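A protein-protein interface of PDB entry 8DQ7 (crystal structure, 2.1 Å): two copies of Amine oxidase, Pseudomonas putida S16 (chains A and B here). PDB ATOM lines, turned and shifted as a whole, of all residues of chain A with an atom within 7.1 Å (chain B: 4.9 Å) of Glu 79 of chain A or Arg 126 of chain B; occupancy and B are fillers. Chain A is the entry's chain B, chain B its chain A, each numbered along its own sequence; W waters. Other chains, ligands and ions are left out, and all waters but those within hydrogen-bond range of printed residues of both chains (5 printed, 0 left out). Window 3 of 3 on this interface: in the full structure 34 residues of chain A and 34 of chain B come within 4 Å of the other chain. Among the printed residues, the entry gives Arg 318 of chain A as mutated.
Water W1 lies within hydrogen-bond range of O of Pro 125 of chain B (2.6 Å), OH of Tyr 202 of chain A (2.6 Å) and OD2 of Asp 197 of chain A (2.7 Å). Water W4 lies within hydrogen-bond range of a ring nitrogen (NE2) of His 128 of chain B and the backbone carbonyl oxygen (O) of Trp 61 of chain A. Water W3 lies within hydrogen-bond range of the side-chain hydroxyl (OH) of Tyr 202 of chain A (2.8 Å), the side-chain carboxylate (OE1) of Glu 79 of chain A (2.9 Å) and the guanidinium group (NE) of Arg 126 of chain B (3.0 Å). Water W5 bridges the backbone carbonyl oxygen of Val 77 of chain A and the guanidinium group of Arg 126 of chain B. Water W2 bridges OE2 of Glu 129 of chain B and N of Val 77 of chain A.
Among the printed residues, pairs that only touch across the chains: Trp 61 of chain A with Pro 125 of chain B (3.3 Å), Trp 61 of chain A with Arg 126 of chain B (3.98 Å), Trp 61 of chain A with Pro 127 of chain B (3.6 Å), Trp 61 of chain A with His 128 of chain B (3.6 Å), Val 77 of chain A with Arg 126 of chain B (3.6 Å), Tyr 202 of chain A with Pro 125 of chain B (3.9 Å) and Tyr 202 of chain A with Arg 126 of chain B (3.8 Å).
Printed residues of chain A that touch a printed residue of chain B: Trp 61, Val 77, Glu 79 and Tyr 202. Hydrophobic or aromatic side chains of chain A within 4 Å of the printed part of chain B: Trp 61, Val 77 and Tyr 202. Printed residues of chain B that touch a printed residue of chain A: Pro 125, Arg 126, Pro 127 and His 128. Hydrophobic or aromatic side chains of chain B within 4 Å of the printed part of chain A: Pro 127 and His 128. Among the printed residues, Asp or Glu carboxylates within 4 Å of a Lys or Arg side-chain nitrogen of the other chain: Glu 79 of chain A with Arg 126 of chain B (3.0 Å).
The side-chain carboxylate of Glu 79 of chain A is in hydrogen-bond range of a ring nitrogen (NE2) of His 201 of chain A. The guanidinium group (NH1) of Arg 126 of chain B is in salt-bridge range of the side-chain carboxylate (OE2) of Glu 129 of chain B (3.0 Å).
No position is printed for both chains.
The guanidinium group (NH2) of Arg 126 of chain B lies within salt-bridge range of the side-chain carboxylate (OE1) of Glu 79 of chain A, at 3.0 Å.
Of the printed residues of chain B, Val 77 of chain A touches Arg 126 (3.6 Å). Glu 79 of chain A touches one residue of chain B. Of the printed residues of chain B, Tyr 202 of chain A touches Pro 125 (3.9 Å) and Arg 126 (3.8 Å). Of the printed residues of chain A, Arg 126 of chain B touches Trp 61 (3.98 Å), Val 77 (3.6 Å), Glu 79 (3.0 Å) and Tyr 202 (3.8 Å). Of the printed residues of chain A, Pro 127 of chain B touches Trp 61 (3.6 Å). Printed residues of chain A within 4 Å of His 128 of chain B: Trp 61. The nearest printed residue of chain A that does not touch His 128 of chain B is Val 77 of chain A (7.9 Å).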
ATOM      1  N   TRP A  58      -8.143 -13.153  17.372  1.00  0.00           N
ATOM      2  CA  TRP A  58      -7.195 -12.948  18.466  1.00  0.00           C
ATOM      3  C   TRP A  58      -7.736 -11.927  19.478  1.00  0.00           C
ATOM      4  O   TRP A  58      -8.411 -10.966  19.107  1.00  0.00           O
ATOM      5  CB  TRP A  58      -5.823 -12.496  17.934  1.00  0.00           C
ATOM      6  CG  TRP A  58      -5.143 -13.535  17.014  1.00  0.00           C
ATOM      7  CD1 TRP A  58      -4.530 -14.724  17.392  1.00  0.00           C
ATOM      8  CD2 TRP A  58      -5.052 -13.483  15.571  1.00  0.00           C
ATOM      9  NE1 TRP A  58      -4.054 -15.393  16.264  1.00  0.00           N
ATOM     10  CE2 TRP A  58      -4.360 -14.652  15.145  1.00  0.00           C
ATOM     11  CE3 TRP A  58      -5.476 -12.559  14.612  1.00  0.00           C
ATOM     12  CZ2 TRP A  58      -4.081 -14.906  13.801  1.00  0.00           C
ATOM     13  CZ3 TRP A  58      -5.201 -12.810  13.267  1.00  0.00           C
ATOM     14  CH2 TRP A  58      -4.501 -13.983  12.875  1.00  0.00           C
ATOM     15  N   TRP A  61      -5.738  -9.720  27.245  1.00  0.00           N
ATOM     16  CA  TRP A  61      -6.189  -9.325  28.579  1.00  0.00           C
ATOM     17  C   TRP A  61      -6.216  -7.810  28.763  1.00  0.00           C
ATOM     18  O   TRP A  61      -6.837  -7.336  29.719  1.00  0.00           O
ATOM     19  CB  TRP A  61      -5.320  -9.965  29.667  1.00  0.00           C
ATOM     20  CG  TRP A  61      -3.870  -9.803  29.450  1.00  0.00           C
ATOM     21  CD1 TRP A  61      -3.087  -8.749  29.849  1.00  0.00           C
ATOM     22  CD2 TRP A  61      -2.999 -10.711  28.734  1.00  0.00           C
ATOM     23  NE1 TRP A  61      -1.783  -8.946  29.438  1.00  0.00           N
ATOM     24  CE2 TRP A  61      -1.699 -10.148  28.765  1.00  0.00           C
ATOM     25  CE3 TRP A  61      -3.195 -11.961  28.099  1.00  0.00           C
ATOM     26  CZ2 TRP A  61      -0.599 -10.770  28.177  1.00  0.00           C
ATOM     27  CZ3 TRP A  61      -2.101 -12.581  27.497  1.00  0.00           C
ATOM     28  CH2 TRP A  61      -0.806 -11.984  27.542  1.00  0.00           C
ATOM     29  N   GLY A  76      -9.139 -20.017  28.856  1.00  0.00           N
ATOM     30  CA  GLY A  76      -7.755 -19.588  28.758  1.00  0.00           C
ATOM     31  C   GLY A  76      -7.426 -19.000  27.383  1.00  0.00           C
ATOM     32  O   GLY A  76      -8.283 -18.822  26.513  1.00  0.00           O
ATOM     33  N   VAL A  77      -6.138 -18.706  27.191  1.00  0.00           N
ATOM     34  CA  VAL A  77      -5.633 -18.261  25.894  1.00  0.00           C
ATOM     35  C   VAL A  77      -4.904 -19.418  25.255  1.00  0.00           C
ATOM     36  O   VAL A  77      -4.360 -20.281  25.940  1.00  0.00           O
ATOM     37  CB  VAL A  77      -4.703 -17.031  25.967  1.00  0.00           C
ATOM     38  CG1 VAL A  77      -5.479 -15.816  26.416  1.00  0.00           C
ATOM     39  CG2 VAL A  77      -3.446 -17.308  26.866  1.00  0.00           C
ATOM     40  N   VAL A  78      -4.838 -19.383  23.933  1.00  0.00           N
ATOM     41  CA  VAL A  78      -4.103 -20.343  23.117  1.00  0.00           C
ATOM     42  C   VAL A  78      -3.118 -19.529  22.279  1.00  0.00           C
ATOM     43  O   VAL A  78      -3.522 -18.667  21.484  1.00  0.00           O
ATOM     44  CB  VAL A  78      -5.058 -21.169  22.220  1.00  0.00           C
ATOM     45  CG1 VAL A  78      -4.276 -22.191  21.366  1.00  0.00           C
ATOM     46  CG2 VAL A  78      -6.093 -21.891  23.064  1.00  0.00           C
ATOM     47  N   GLU A  79      -1.826 -19.781  22.456  1.00  0.00           N
ATOM     48  CA  GLU A  79      -0.813 -18.911  21.866  1.00  0.00           C
ATOM     49  C   GLU A  79      -0.485 -19.355  20.446  1.00  0.00           C
ATOM     50  O   GLU A  79      -0.090 -20.514  20.239  1.00  0.00           O
ATOM     51  CB  GLU A  79       0.453 -18.914  22.724  1.00  0.00           C
ATOM     52  CG  GLU A  79       1.420 -17.874  22.268  1.00  0.00           C
ATOM     53  CD  GLU A  79       2.724 -17.885  23.058  1.00  0.00           C
ATOM     54  OE1 GLU A  79       2.764 -18.460  24.159  1.00  0.00           O
ATOM     55  OE2 GLU A  79       3.706 -17.323  22.550  1.00  0.00           O
ATOM     56  N   ASP A  80      -0.635 -18.416  19.444  1.00  0.00           N
ATOM     57  CA  ASP A  80      -0.101 -18.697  18.112  1.00  0.00           C
ATOM     58  C   ASP A  80       1.364 -18.314  18.045  1.00  0.00           C
ATOM     59  O   ASP A  80       1.860 -17.493  18.839  1.00  0.00           O
ATOM     60  CB  ASP A  80      -0.890 -17.954  17.032  1.00  0.00           C
ATOM     61  CG  ASP A  80      -2.205 -18.626  16.721  1.00  0.00           C
ATOM     62  OD1 ASP A  80      -2.312 -19.852  16.947  1.00  0.00           O
ATOM     63  OD2 ASP A  80      -3.154 -17.930  16.296  1.00  0.00           O
ATOM     64  N   PRO A  81       2.116 -18.927  17.103  1.00  0.00           N
ATOM     65  CA  PRO A  81       3.606 -18.755  17.100  1.00  0.00           C
ATOM     66  C   PRO A  81       4.064 -17.417  16.529  1.00  0.00           C
ATOM     67  O   PRO A  81       4.553 -17.332  15.428  1.00  0.00           O
ATOM     68  CB  PRO A  81       4.068 -19.906  16.199  1.00  0.00           C
ATOM     69  CG  PRO A  81       2.900 -20.186  15.255  1.00  0.00           C
ATOM     70  CD  PRO A  81       1.652 -19.921  16.113  1.00  0.00           C
ATOM     71  N   LEU A  82       3.915 -16.346  17.337  1.00  0.00           N
ATOM     72  CA  LEU A  82       4.326 -14.993  16.936  1.00  0.00           C
ATOM     73  C   LEU A  82       5.709 -14.597  17.445  1.00  0.00           C
ATOM     74  O   LEU A  82       6.266 -13.608  16.957  1.00  0.00           O
ATOM     75  CB  LEU A  82       3.303 -13.948  17.426  1.00  0.00           C
ATOM     76  N   THR A  83       6.263 -15.319  18.421  1.00  0.00           N
ATOM     77  CA  THR A  83       7.584 -15.020  18.958  1.00  0.00           C
ATOM     78  C   THR A  83       8.627 -15.927  18.318  1.00  0.00           C
ATOM     79  O   THR A  83       8.306 -16.965  17.736  1.00  0.00           O
ATOM     80  CB  THR A  83       7.604 -15.212  20.479  1.00  0.00           C
ATOM     81  OG1 THR A  83       7.354 -16.594  20.774  1.00  0.00           O
ATOM     82  CG2 THR A  83       6.532 -14.378  21.129  1.00  0.00           C
ATOM     83  N   ASP A 197       0.955  -6.793  20.740  1.00  0.00           N
ATOM     84  CA  ASP A 197       0.630  -8.037  21.420  1.00  0.00           C
ATOM     85  C   ASP A 197      -0.875  -8.303  21.461  1.00  0.00           C
ATOM     86  O   ASP A 197      -1.296  -9.472  21.454  1.00  0.00           O
ATOM     87  CB  ASP A 197       1.206  -8.015  22.838  1.00  0.00           C
ATOM     88  CG  ASP A 197       1.453  -9.405  23.373  1.00  0.00           C
ATOM     89  OD1 ASP A 197       1.981 -10.226  22.597  1.00  0.00           O
ATOM     90  OD2 ASP A 197       1.120  -9.686  24.579  1.00  0.00           O
ATOM     91  N   HIS A 201      -1.820 -12.464  18.641  1.00  0.00           N
ATOM     92  CA  HIS A 201      -0.993 -13.385  19.419  1.00  0.00           C
ATOM     93  C   HIS A 201      -1.780 -14.494  20.111  1.00  0.00           C
ATOM     94  O   HIS A 201      -1.366 -15.647  20.032  1.00  0.00           O
ATOM     95  CB  HIS A 201      -0.175 -12.584  20.440  1.00  0.00           C
ATOM     96  CG  HIS A 201       1.020 -13.316  20.997  1.00  0.00           C
ATOM     97  ND1 HIS A 201       1.875 -12.743  21.939  1.00  0.00           N
ATOM     98  CD2 HIS A 201       1.519 -14.553  20.729  1.00  0.00           C
ATOM     99  CE1 HIS A 201       2.821 -13.621  22.251  1.00  0.00           C
ATOM    100  NE2 HIS A 201       2.632 -14.721  21.532  1.00  0.00           N
ATOM    101  N   TYR A 202      -2.899 -14.181  20.802  1.00  0.00           N
ATOM    102  CA  TYR A 202      -3.618 -15.154  21.607  1.00  0.00           C
ATOM    103  C   TYR A 202      -5.026 -15.379  21.074  1.00  0.00           C
ATOM    104  O   TYR A 202      -5.736 -14.415  20.746  1.00  0.00           O
ATOM    105  CB  TYR A 202      -3.689 -14.661  23.080  1.00  0.00           C
ATOM    106  CG  TYR A 202      -2.320 -14.476  23.676  1.00  0.00           C
ATOM    107  CD1 TYR A 202      -1.587 -15.585  24.088  1.00  0.00           C
ATOM    108  CD2 TYR A 202      -1.741 -13.215  23.807  1.00  0.00           C
ATOM    109  CE1 TYR A 202      -0.337 -15.455  24.624  1.00  0.00           C
ATOM    110  CE2 TYR A 202      -0.463 -13.060  24.369  1.00  0.00           C
ATOM    111  CZ  TYR A 202       0.226 -14.200  24.768  1.00  0.00           C
ATOM    112  OH  TYR A 202       1.483 -14.134  25.302  1.00  0.00           O
ATOM    113  N   ARG A 203      -5.435 -16.661  21.004  1.00  0.00           N
ATOM    114  CA  ARG A 203      -6.788 -17.041  20.625  1.00  0.00           C
ATOM    115  C   ARG A 203      -7.554 -17.471  21.873  1.00  0.00           C
ATOM    116  O   ARG A 203      -6.976 -17.737  22.916  1.00  0.00           O
ATOM    117  CB  ARG A 203      -6.784 -18.191  19.598  1.00  0.00           C
ATOM    118  CG  ARG A 203      -6.569 -17.772  18.163  1.00  0.00           C
ATOM    119  CD  ARG A 203      -6.586 -18.984  17.218  1.00  0.00           C
ATOM    120  NE  ARG A 203      -5.355 -19.761  17.318  1.00  0.00           N
ATOM    121  CZ  ARG A 203      -5.286 -21.031  17.687  1.00  0.00           C
ATOM    122  NH1 ARG A 203      -6.367 -21.711  18.038  1.00  0.00           N
ATOM    123  NH2 ARG A 203      -4.098 -21.635  17.714  1.00  0.00           N
ATOM    124  N   ARG A 301       7.927 -20.568  11.674  1.00  0.00           N
ATOM    125  CA  ARG A 301       7.175 -19.439  12.219  1.00  0.00           C
ATOM    126  C   ARG A 301       7.477 -18.210  11.362  1.00  0.00           C
ATOM    127  O   ARG A 301       8.585 -17.640  11.431  1.00  0.00           O
ATOM    128  CB  ARG A 301       7.533 -19.212  13.689  1.00  0.00           C
ATOM    129  CG  ARG A 301       7.546 -20.481  14.526  1.00  0.00           C
ATOM    130  CD  ARG A 301       8.541 -20.372  15.686  1.00  0.00           C
ATOM    131  NE  ARG A 301       8.004 -19.555  16.767  1.00  0.00           N
ATOM    132  CZ  ARG A 301       7.168 -19.994  17.705  1.00  0.00           C
ATOM    133  NH1 ARG A 301       6.768 -21.262  17.750  1.00  0.00           N
ATOM    134  NH2 ARG A 301       6.728 -19.140  18.627  1.00  0.00           N
ATOM    135  N   ARG A 318      -0.227 -20.305  11.387  1.00  0.00           N
ATOM    136  CA  ARG A 318      -1.195 -20.898  12.310  1.00  0.00           C
ATOM    137  C   ARG A 318      -0.741 -22.254  12.850  1.00  0.00           C
ATOM    138  O   ARG A 318      -1.090 -22.604  13.995  1.00  0.00           O
ATOM    139  CB  ARG A 318      -2.553 -21.048  11.623  1.00  0.00           C
ATOM    140  CG  ARG A 318      -3.502 -22.070  12.265  1.00  0.00           C
ATOM    141  CD  ARG A 318      -4.081 -21.553  13.607  1.00  0.00           C
ATOM    142  NE  ARG A 318      -5.045 -22.491  14.174  1.00  0.00           N
ATOM    143  CZ  ARG A 318      -4.718 -23.619  14.790  1.00  0.00           C
ATOM    144  NH1 ARG A 318      -3.454 -24.003  14.918  1.00  0.00           N
ATOM    145  NH2 ARG A 318      -5.676 -24.381  15.299  1.00  0.00           N
ATOM    146  N   PHE B 124       7.268 -11.732  32.554  1.00  0.00           N
ATOM    147  CA  PHE B 124       5.813 -11.782  32.668  1.00  0.00           C
ATOM    148  C   PHE B 124       5.176 -11.504  31.320  1.00  0.00           C
ATOM    149  O   PHE B 124       4.378 -10.568  31.163  1.00  0.00           O
ATOM    150  CB  PHE B 124       5.316 -10.801  33.731  1.00  0.00           C
ATOM    151  CG  PHE B 124       5.596 -11.265  35.152  1.00  0.00           C
ATOM    152  CD1 PHE B 124       4.851 -12.287  35.712  1.00  0.00           C
ATOM    153  CD2 PHE B 124       6.610 -10.701  35.894  1.00  0.00           C
ATOM    154  CE1 PHE B 124       5.106 -12.747  36.988  1.00  0.00           C
ATOM    155  CE2 PHE B 124       6.878 -11.136  37.184  1.00  0.00           C
ATOM    156  CZ  PHE B 124       6.118 -12.176  37.737  1.00  0.00           C
ATOM    157  N   PRO B 125       5.449 -12.344  30.329  1.00  0.00           N
ATOM    158  CA  PRO B 125       4.740 -12.187  29.058  1.00  0.00           C
ATOM    159  C   PRO B 125       3.245 -12.409  29.213  1.00  0.00           C
ATOM    160  O   PRO B 125       2.465 -11.940  28.371  1.00  0.00           O
ATOM    161  CB  PRO B 125       5.390 -13.251  28.137  1.00  0.00           C
ATOM    162  CG  PRO B 125       5.896 -14.327  29.099  1.00  0.00           C
ATOM    163  CD  PRO B 125       6.219 -13.610  30.417  1.00  0.00           C
ATOM    164  N   ARG B 126       2.824 -13.120  30.258  1.00  0.00           N
ATOM    165  CA  ARG B 126       1.422 -13.462  30.492  1.00  0.00           C
ATOM    166  C   ARG B 126       1.127 -13.143  31.954  1.00  0.00           C
ATOM    167  O   ARG B 126       1.081 -14.061  32.803  1.00  0.00           O
ATOM    168  CB  ARG B 126       1.145 -14.942  30.247  1.00  0.00           C
ATOM    169  CG  ARG B 126       1.290 -15.458  28.868  1.00  0.00           C
ATOM    170  CD  ARG B 126       0.590 -16.832  28.831  1.00  0.00           C
ATOM    171  NE  ARG B 126       0.965 -17.607  27.654  1.00  0.00           N
ATOM    172  CZ  ARG B 126       0.388 -18.753  27.311  1.00  0.00           C
ATOM    173  NH1 ARG B 126      -0.609 -19.274  28.022  1.00  0.00           N
ATOM    174  NH2 ARG B 126       0.837 -19.400  26.241  1.00  0.00           N
ATOM    175  N   PRO B 127       0.922 -11.870  32.292  1.00  0.00           N
ATOM    176  CA  PRO B 127       0.839 -11.499  33.727  1.00  0.00           C
ATOM    177  C   PRO B 127      -0.290 -12.159  34.477  1.00  0.00           C
ATOM    178  O   PRO B 127      -0.241 -12.191  35.719  1.00  0.00           O
ATOM    179  CB  PRO B 127       0.668  -9.968  33.701  1.00  0.00           C
ATOM    180  CG  PRO B 127       0.252  -9.608  32.314  1.00  0.00           C
ATOM    181  CD  PRO B 127       0.880 -10.697  31.405  1.00  0.00           C
ATOM    182  N   HIS B 128      -1.322 -12.678  33.794  1.00  0.00           N
ATOM    183  CA  HIS B 128      -2.389 -13.413  34.482  1.00  0.00           C
ATOM    184  C   HIS B 128      -2.042 -14.877  34.711  1.00  0.00           C
ATOM    185  O   HIS B 128      -2.901 -15.629  35.201  1.00  0.00           O
ATOM    186  CB  HIS B 128      -3.727 -13.317  33.704  1.00  0.00           C
ATOM    187  CG  HIS B 128      -4.281 -11.934  33.707  1.00  0.00           C
ATOM    188  ND1 HIS B 128      -5.087 -11.460  34.730  1.00  0.00           N
ATOM    189  CD2 HIS B 128      -4.052 -10.887  32.883  1.00  0.00           C
ATOM    190  CE1 HIS B 128      -5.377 -10.192  34.487  1.00  0.00           C
ATOM    191  NE2 HIS B 128      -4.746  -9.818  33.386  1.00  0.00           N
ATOM    192  N   GLU B 129      -0.838 -15.290  34.337  1.00  0.00           N
ATOM    193  CA  GLU B 129      -0.290 -16.606  34.685  1.00  0.00           C
ATOM    194  C   GLU B 129       1.056 -16.307  35.331  1.00  0.00           C
ATOM    195  O   GLU B 129       2.119 -16.428  34.697  1.00  0.00           O
ATOM    196  CB  GLU B 129      -0.141 -17.517  33.445  1.00  0.00           C
ATOM    197  CG  GLU B 129      -1.450 -18.172  32.932  1.00  0.00           C
ATOM    198  CD  GLU B 129      -1.316 -18.775  31.494  1.00  0.00           C
ATOM    199  OE1 GLU B 129      -0.728 -19.857  31.392  1.00  0.00           O
ATOM    200  OE2 GLU B 129      -1.842 -18.204  30.489  1.00  0.00           O
ATOM    201  N   PRO B 130       1.049 -15.918  36.601  1.00  0.00           N
ATOM    202  CA  PRO B 130       2.265 -15.305  37.185  1.00  0.00           C
ATOM    203  C   PRO B 130       3.484 -16.216  37.165  1.00  0.00           C
ATOM    204  O   PRO B 130       4.607 -15.726  37.024  1.00  0.00           O
ATOM    205  CB  PRO B 130       1.832 -14.970  38.622  1.00  0.00           C
ATOM    206  CG  PRO B 130       0.340 -14.881  38.551  1.00  0.00           C
ATOM    207  CD  PRO B 130      -0.082 -15.931  37.551  1.00  0.00           C
ATOM    208  N   PHE B 132       4.158 -18.458  34.777  1.00  0.00           N
ATOM    209  CA  PHE B 132       4.331 -19.008  33.438  1.00  0.00           C
ATOM    210  C   PHE B 132       5.802 -19.282  33.133  1.00  0.00           C
ATOM    211  O   PHE B 132       6.127 -20.319  32.547  1.00  0.00           O
ATOM    212  CB  PHE B 132       3.712 -18.058  32.400  1.00  0.00           C
ATOM    213  CG  PHE B 132       3.714 -18.598  30.969  1.00  0.00           C
ATOM    214  CD1 PHE B 132       2.953 -19.696  30.623  1.00  0.00           C
ATOM    215  CD2 PHE B 132       4.452 -17.957  29.977  1.00  0.00           C
ATOM    216  CE1 PHE B 132       2.905 -20.174  29.292  1.00  0.00           C
ATOM    217  CE2 PHE B 132       4.435 -18.416  28.647  1.00  0.00           C
ATOM    218  CZ  PHE B 132       3.661 -19.537  28.301  1.00  0.00           C
HETATM  219  O   HOH W   1       2.484 -11.724  25.752  1.00  0.00           O
HETATM  220  O   HOH W   2      -4.545 -19.118  29.664  1.00  0.00           O
HETATM  221  O   HOH W   3       3.108 -16.262  26.096  1.00  0.00           O
HETATM  222  O   HOH W   4      -5.503  -7.550  32.144  1.00  0.00           O
HETATM  223  O   HOH W   5      -1.966 -21.540  26.770  1.00  0.00           O
